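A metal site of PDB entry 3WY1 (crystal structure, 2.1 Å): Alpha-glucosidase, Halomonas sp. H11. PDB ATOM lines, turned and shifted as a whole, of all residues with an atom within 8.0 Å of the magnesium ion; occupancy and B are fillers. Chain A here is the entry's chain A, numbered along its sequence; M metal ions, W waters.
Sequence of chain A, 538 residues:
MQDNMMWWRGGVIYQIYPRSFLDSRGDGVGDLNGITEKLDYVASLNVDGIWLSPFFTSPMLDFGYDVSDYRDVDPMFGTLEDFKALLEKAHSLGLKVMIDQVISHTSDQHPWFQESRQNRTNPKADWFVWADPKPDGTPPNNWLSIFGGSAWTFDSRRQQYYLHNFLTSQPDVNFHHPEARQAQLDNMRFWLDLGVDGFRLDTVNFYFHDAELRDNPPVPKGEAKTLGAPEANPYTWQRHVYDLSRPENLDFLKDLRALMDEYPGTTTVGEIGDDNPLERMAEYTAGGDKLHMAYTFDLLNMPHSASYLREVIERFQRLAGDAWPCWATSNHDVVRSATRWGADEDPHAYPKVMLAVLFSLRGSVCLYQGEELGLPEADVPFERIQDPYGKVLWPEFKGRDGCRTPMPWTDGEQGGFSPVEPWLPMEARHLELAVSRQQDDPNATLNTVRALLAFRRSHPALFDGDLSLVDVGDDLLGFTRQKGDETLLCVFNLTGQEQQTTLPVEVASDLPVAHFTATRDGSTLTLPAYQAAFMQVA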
ATOM      1  N   PRO A  18       8.007  -7.752 -10.790  1.00  0.00           N
ATOM      2  CA  PRO A  18       8.441  -8.267  -9.480  1.00  0.00           C
ATOM      3  C   PRO A  18       7.883  -9.640  -9.113  1.00  0.00           C
ATOM      4  O   PRO A  18       8.663 -10.444  -8.607  1.00  0.00           O
ATOM      5  CB  PRO A  18       7.941  -7.181  -8.501  1.00  0.00           C
ATOM      6  CG  PRO A  18       7.992  -5.922  -9.324  1.00  0.00           C
ATOM      7  CD  PRO A  18       7.582  -6.352 -10.718  1.00  0.00           C
ATOM      8  N   ARG A  19       6.598  -9.895  -9.366  1.00  0.00           N
ATOM      9  CA  ARG A  19       5.952 -11.177  -9.049  1.00  0.00           C
ATOM     10  C   ARG A  19       6.656 -12.394  -9.640  1.00  0.00           C
ATOM     11  O   ARG A  19       6.572 -13.501  -9.078  1.00  0.00           O
ATOM     12  CB  ARG A  19       4.541 -11.229  -9.620  1.00  0.00           C
ATOM     13  CG  ARG A  19       3.483 -10.467  -8.882  1.00  0.00           C
ATOM     14  CD  ARG A  19       2.123 -10.848  -9.450  1.00  0.00           C
ATOM     15  NE  ARG A  19       1.690 -12.133  -8.888  1.00  0.00           N
ATOM     16  CZ  ARG A  19       1.122 -12.254  -7.691  1.00  0.00           C
ATOM     17  NH1 ARG A  19       0.919 -11.180  -6.934  1.00  0.00           N
ATOM     18  NH2 ARG A  19       0.760 -13.440  -7.248  1.00  0.00           N
ATOM     19  N   LEU A  22      12.141 -13.243  -9.020  1.00  0.00           N
ATOM     20  CA  LEU A  22      12.755 -14.220  -8.114  1.00  0.00           C
ATOM     21  C   LEU A  22      12.106 -14.232  -6.725  1.00  0.00           C
ATOM     22  O   LEU A  22      11.992 -13.206  -6.064  1.00  0.00           O
ATOM     23  CB  LEU A  22      14.254 -13.965  -7.956  1.00  0.00           C
ATOM     24  CG  LEU A  22      14.945 -14.967  -7.022  1.00  0.00           C
ATOM     25  CD1 LEU A  22      14.855 -16.397  -7.588  1.00  0.00           C
ATOM     26  CD2 LEU A  22      16.387 -14.570  -6.746  1.00  0.00           C
ATOM     27  N   ASP A  23      11.684 -15.425  -6.300  1.00  0.00           N
ATOM     28  CA  ASP A  23      11.116 -15.630  -4.968  1.00  0.00           C
ATOM     29  C   ASP A  23      12.249 -15.972  -4.000  1.00  0.00           C
ATOM     30  O   ASP A  23      12.860 -17.036  -4.116  1.00  0.00           O
ATOM     31  CB  ASP A  23      10.082 -16.755  -5.012  1.00  0.00           C
ATOM     32  CG  ASP A  23       9.611 -17.190  -3.622  1.00  0.00           C
ATOM     33  OD1 ASP A  23       9.571 -16.358  -2.686  1.00  0.00           O
ATOM     34  OD2 ASP A  23       9.268 -18.384  -3.473  1.00  0.00           O
ATOM     35  N   SER A  24      12.534 -15.072  -3.073  1.00  0.00           N
ATOM     36  CA  SER A  24      13.613 -15.323  -2.123  1.00  0.00           C
ATOM     37  C   SER A  24      13.087 -15.816  -0.772  1.00  0.00           C
ATOM     38  O   SER A  24      13.872 -16.210   0.096  1.00  0.00           O
ATOM     39  CB  SER A  24      14.437 -14.052  -1.903  1.00  0.00           C
ATOM     40  OG  SER A  24      13.668 -13.063  -1.244  1.00  0.00           O
ATOM     41  N   ARG A  25      11.777 -15.791  -0.587  1.00  0.00           N
ATOM     42  CA  ARG A  25      11.222 -16.137   0.723  1.00  0.00           C
ATOM     43  C   ARG A  25      10.512 -17.500   0.772  1.00  0.00           C
ATOM     44  O   ARG A  25      10.432 -18.125   1.831  1.00  0.00           O
ATOM     45  CB  ARG A  25      10.350 -15.013   1.288  1.00  0.00           C
ATOM     46  CG  ARG A  25       9.929 -15.251   2.733  1.00  0.00           C
ATOM     47  CD  ARG A  25       8.957 -14.210   3.247  1.00  0.00           C
ATOM     48  NE  ARG A  25       9.550 -12.866   3.169  1.00  0.00           N
ATOM     49  CZ  ARG A  25       9.049 -11.795   3.771  1.00  0.00           C
ATOM     50  NH1 ARG A  25       7.954 -11.882   4.520  1.00  0.00           N
ATOM     51  NH2 ARG A  25       9.658 -10.616   3.643  1.00  0.00           N
ATOM     52  N   GLY A  26      10.009 -17.987  -0.360  1.00  0.00           N
ATOM     53  CA  GLY A  26       9.473 -19.339  -0.429  1.00  0.00           C
ATOM     54  C   GLY A  26       7.963 -19.485  -0.544  1.00  0.00           C
ATOM     55  O   GLY A  26       7.420 -20.564  -0.293  1.00  0.00           O
ATOM     56  N   ASP A  27       7.285 -18.408  -0.943  1.00  0.00           N
ATOM     57  CA  ASP A  27       5.825 -18.439  -1.050  1.00  0.00           C
ATOM     58  C   ASP A  27       5.355 -18.605  -2.505  1.00  0.00           C
ATOM     59  O   ASP A  27       4.159 -18.671  -2.772  1.00  0.00           O
ATOM     60  CB  ASP A  27       5.229 -17.172  -0.447  1.00  0.00           C
ATOM     61  CG  ASP A  27       5.918 -15.912  -0.949  1.00  0.00           C
ATOM     62  OD1 ASP A  27       6.702 -16.014  -1.910  1.00  0.00           O
ATOM     63  OD2 ASP A  27       5.676 -14.835  -0.375  1.00  0.00           O
ATOM     64  N   GLY A  28       6.305 -18.658  -3.439  1.00  0.00           N
ATOM     65  CA  GLY A  28       5.974 -18.864  -4.847  1.00  0.00           C
ATOM     66  C   GLY A  28       5.741 -17.574  -5.629  1.00  0.00           C
ATOM     67  O   GLY A  28       5.424 -17.610  -6.817  1.00  0.00           O
ATOM     68  N   VAL A  29       5.881 -16.449  -4.941  1.00  0.00           N
ATOM     69  CA  VAL A  29       5.720 -15.137  -5.546  1.00  0.00           C
ATOM     70  C   VAL A  29       7.040 -14.394  -5.469  1.00  0.00           C
ATOM     71  O   VAL A  29       7.666 -14.363  -4.413  1.00  0.00           O
ATOM     72  CB  VAL A  29       4.684 -14.298  -4.765  1.00  0.00           C
ATOM     73  CG1 VAL A  29       4.582 -12.874  -5.330  1.00  0.00           C
ATOM     74  CG2 VAL A  29       3.318 -14.974  -4.775  1.00  0.00           C
ATOM     75  N   GLY A  30       7.459 -13.780  -6.578  1.00  0.00           N
ATOM     76  CA  GLY A  30       8.682 -12.992  -6.596  1.00  0.00           C
ATOM     77  C   GLY A  30       8.598 -11.820  -5.635  1.00  0.00           C
ATOM     78  O   GLY A  30       7.534 -11.242  -5.445  1.00  0.00           O
ATOM     79  N   ASP A  31       9.736 -11.470  -5.035  1.00  0.00           N
ATOM     80  CA  ASP A  31       9.776 -10.388  -4.059  1.00  0.00           C
ATOM     81  C   ASP A  31      10.918  -9.425  -4.360  1.00  0.00           C
ATOM     82  O   ASP A  31      11.687  -9.655  -5.294  1.00  0.00           O
ATOM     83  CB  ASP A  31       9.879 -10.948  -2.644  1.00  0.00           C
ATOM     84  CG  ASP A  31      10.897 -12.073  -2.526  1.00  0.00           C
ATOM     85  OD1 ASP A  31      12.096 -11.791  -2.689  1.00  0.00           O
ATOM     86  OD2 ASP A  31      10.487 -13.224  -2.283  1.00  0.00           O
ATOM     87  N   LEU A  32      10.998  -8.344  -3.594  1.00  0.00           N
ATOM     88  CA  LEU A  32      12.029  -7.324  -3.832  1.00  0.00           C
ATOM     89  C   LEU A  32      13.440  -7.827  -3.566  1.00  0.00           C
ATOM     90  O   LEU A  32      14.385  -7.528  -4.308  1.00  0.00           O
ATOM     91  CB  LEU A  32      11.764  -6.105  -2.965  1.00  0.00           C
ATOM     92  CG  LEU A  32      10.549  -5.250  -3.297  1.00  0.00           C
ATOM     93  CD1 LEU A  32      10.561  -3.975  -2.455  1.00  0.00           C
ATOM     94  CD2 LEU A  32      10.495  -4.919  -4.796  1.00  0.00           C
ATOM     95  N   ASN A  33      13.584  -8.599  -2.483  1.00  0.00           N
ATOM     96  CA  ASN A  33      14.889  -9.133  -2.102  1.00  0.00           C
ATOM     97  C   ASN A  33      15.493 -10.056  -3.158  1.00  0.00           C
ATOM     98  O   ASN A  33      16.712 -10.132  -3.275  1.00  0.00           O
ATOM     99  CB  ASN A  33      14.783  -9.849  -0.750  1.00  0.00           C
ATOM    100  CG  ASN A  33      14.534  -8.896   0.401  1.00  0.00           C
ATOM    101  OD1 ASN A  33      14.718  -7.691   0.267  1.00  0.00           O
ATOM    102  ND2 ASN A  33      14.112  -9.429   1.533  1.00  0.00           N
ATOM    103  N   GLY A  34      14.631 -10.751  -3.906  1.00  0.00           N
ATOM    104  CA  GLY A  34      15.069 -11.558  -5.040  1.00  0.00           C
ATOM    105  C   GLY A  34      15.689 -10.705  -6.126  1.00  0.00           C
ATOM    106  O   GLY A  34      16.746 -11.052  -6.691  1.00  0.00           O
ATOM    107  N   PRO A  75       3.030  -6.318   1.673  1.00  0.00           N
ATOM    108  CA  PRO A  75       3.686  -7.342   2.485  1.00  0.00           C
ATOM    109  C   PRO A  75       4.181  -8.524   1.652  1.00  0.00           C
ATOM    110  O   PRO A  75       5.200  -9.134   1.973  1.00  0.00           O
ATOM    111  CB  PRO A  75       2.562  -7.791   3.425  1.00  0.00           C
ATOM    112  CG  PRO A  75       1.777  -6.519   3.638  1.00  0.00           C
ATOM    113  CD  PRO A  75       1.750  -5.879   2.274  1.00  0.00           C
ATOM    114  N   MET A  76       3.459  -8.804   0.568  1.00  0.00           N
ATOM    115  CA  MET A  76       3.790  -9.884  -0.340  1.00  0.00           C
ATOM    116  C   MET A  76       5.127  -9.639  -1.032  1.00  0.00           C
ATOM    117  O   MET A  76       5.847 -10.582  -1.357  1.00  0.00           O
ATOM    118  CB  MET A  76       2.663  -9.957  -1.366  1.00  0.00           C
ATOM    119  CG  MET A  76       2.836 -10.950  -2.465  1.00  0.00           C
ATOM    120  SD  MET A  76       1.510 -10.713  -3.673  1.00  0.00           S
ATOM    121  CE  MET A  76       0.078 -10.539  -2.589  1.00  0.00           C
ATOM    122  N   PHE A  77       5.476  -8.376  -1.251  1.00  0.00           N
ATOM    123  CA  PHE A  77       6.745  -8.061  -1.926  1.00  0.00           C
ATOM    124  C   PHE A  77       7.891  -7.781  -0.965  1.00  0.00           C
ATOM    125  O   PHE A  77       9.055  -7.777  -1.369  1.00  0.00           O
ATOM    126  CB  PHE A  77       6.544  -6.920  -2.933  1.00  0.00           C
ATOM    127  CG  PHE A  77       5.607  -7.282  -4.060  1.00  0.00           C
ATOM    128  CD1 PHE A  77       5.865  -8.366  -4.897  1.00  0.00           C
ATOM    129  CD2 PHE A  77       4.443  -6.545  -4.268  1.00  0.00           C
ATOM    130  CE1 PHE A  77       4.993  -8.696  -5.929  1.00  0.00           C
ATOM    131  CE2 PHE A  77       3.561  -6.884  -5.298  1.00  0.00           C
ATOM    132  CZ  PHE A  77       3.829  -7.954  -6.121  1.00  0.00           C
ATOM    133  N   GLY A  78       7.559  -7.532   0.295  1.00  0.00           N
ATOM    134  CA  GLY A  78       8.556  -7.245   1.302  1.00  0.00           C
ATOM    135  C   GLY A  78       8.208  -5.998   2.079  1.00  0.00           C
ATOM    136  O   GLY A  78       7.046  -5.759   2.426  1.00  0.00           O
ATOM    137  N   PHE A 417      13.409 -20.715  -9.650  1.00  0.00           N
ATOM    138  CA  PHE A 417      12.660 -19.507  -9.324  1.00  0.00           C
ATOM    139  C   PHE A 417      12.106 -19.516  -7.902  1.00  0.00           C
ATOM    140  O   PHE A 417      12.068 -18.476  -7.254  1.00  0.00           O
ATOM    141  CB  PHE A 417      11.509 -19.269 -10.327  1.00  0.00           C
ATOM    142  CG  PHE A 417      10.524 -18.225  -9.868  1.00  0.00           C
ATOM    143  CD1 PHE A 417      10.852 -16.870  -9.930  1.00  0.00           C
ATOM    144  CD2 PHE A 417       9.291 -18.602  -9.331  1.00  0.00           C
ATOM    145  CE1 PHE A 417       9.961 -15.907  -9.484  1.00  0.00           C
ATOM    146  CE2 PHE A 417       8.387 -17.634  -8.888  1.00  0.00           C
ATOM    147  CZ  PHE A 417       8.731 -16.280  -8.960  1.00  0.00           C
ATOM    148  N   SER A 418      11.695 -20.704  -7.442  1.00  0.00           N
ATOM    149  CA  SER A 418      11.065 -20.845  -6.138  1.00  0.00           C
ATOM    150  C   SER A 418      11.189 -22.276  -5.630  1.00  0.00           C
ATOM    151  O   SER A 418      11.211 -23.214  -6.419  1.00  0.00           O
ATOM    152  CB  SER A 418       9.578 -20.494  -6.232  1.00  0.00           C
ATOM    153  OG  SER A 418       8.954 -20.655  -4.971  1.00  0.00           O
ATOM    154  N   PRO A 419      11.268 -22.444  -4.291  1.00  0.00           N
ATOM    155  CA  PRO A 419      11.290 -23.768  -3.657  1.00  0.00           C
ATOM    156  C   PRO A 419       9.915 -24.415  -3.646  1.00  0.00           C
ATOM    157  O   PRO A 419       9.822 -25.615  -3.394  1.00  0.00           O
ATOM    158  CB  PRO A 419      11.728 -23.471  -2.226  1.00  0.00           C
ATOM    159  CG  PRO A 419      11.275 -22.064  -2.000  1.00  0.00           C
ATOM    160  CD  PRO A 419      11.474 -21.364  -3.302  1.00  0.00           C
HETATM  161 MG    MG M   1       8.358 -14.367  -2.303  1.00  0.00          MG
HETATM  162  O   HOH W   1       7.346 -13.066  -1.048  1.00  0.00           O
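OD2 of Asp 23 lies close to N of Gly 26 (3.2 Å).
N of Gly 28 sits at hydrogen-bond distance from OD2 of Asp 23 (3.0 Å).
The side-chain carboxylate of Asp 23 lies within hydrogen-bond range of the side-chain hydroxyl of Ser 418 (2.7 Å).
N of Asp 23 is in hydrogen-bond range of O of Phe 417 (3.2 Å).
The backbone NH of Arg 25 lies close to the side-chain carboxylate of Asp 31 (3.3 Å).
OD1 of Asp 31 sits at hydrogen-bond distance from OG of Ser 24.
The backbone carbonyl oxygen (O) of Leu 22 is in hydrogen-bond range of the backbone NH (N) of Asp 31 (3.0 Å).
The backbone NH of Gly 34 sits at hydrogen-bond distance from the side-chain carboxylate of Asp 31.
The magnesium ion is bound by water W1 (2.1 Å), O of Val 29 (2.2 Å), OD1 of Asp 23 (2.4 Å), OD1 of Asp 27 (2.4 Å) and OD2 of Asp 31 (2.4 Å).
Water W1 lies within hydrogen-bond range of OD2 of Asp 27 and O of Met 76.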
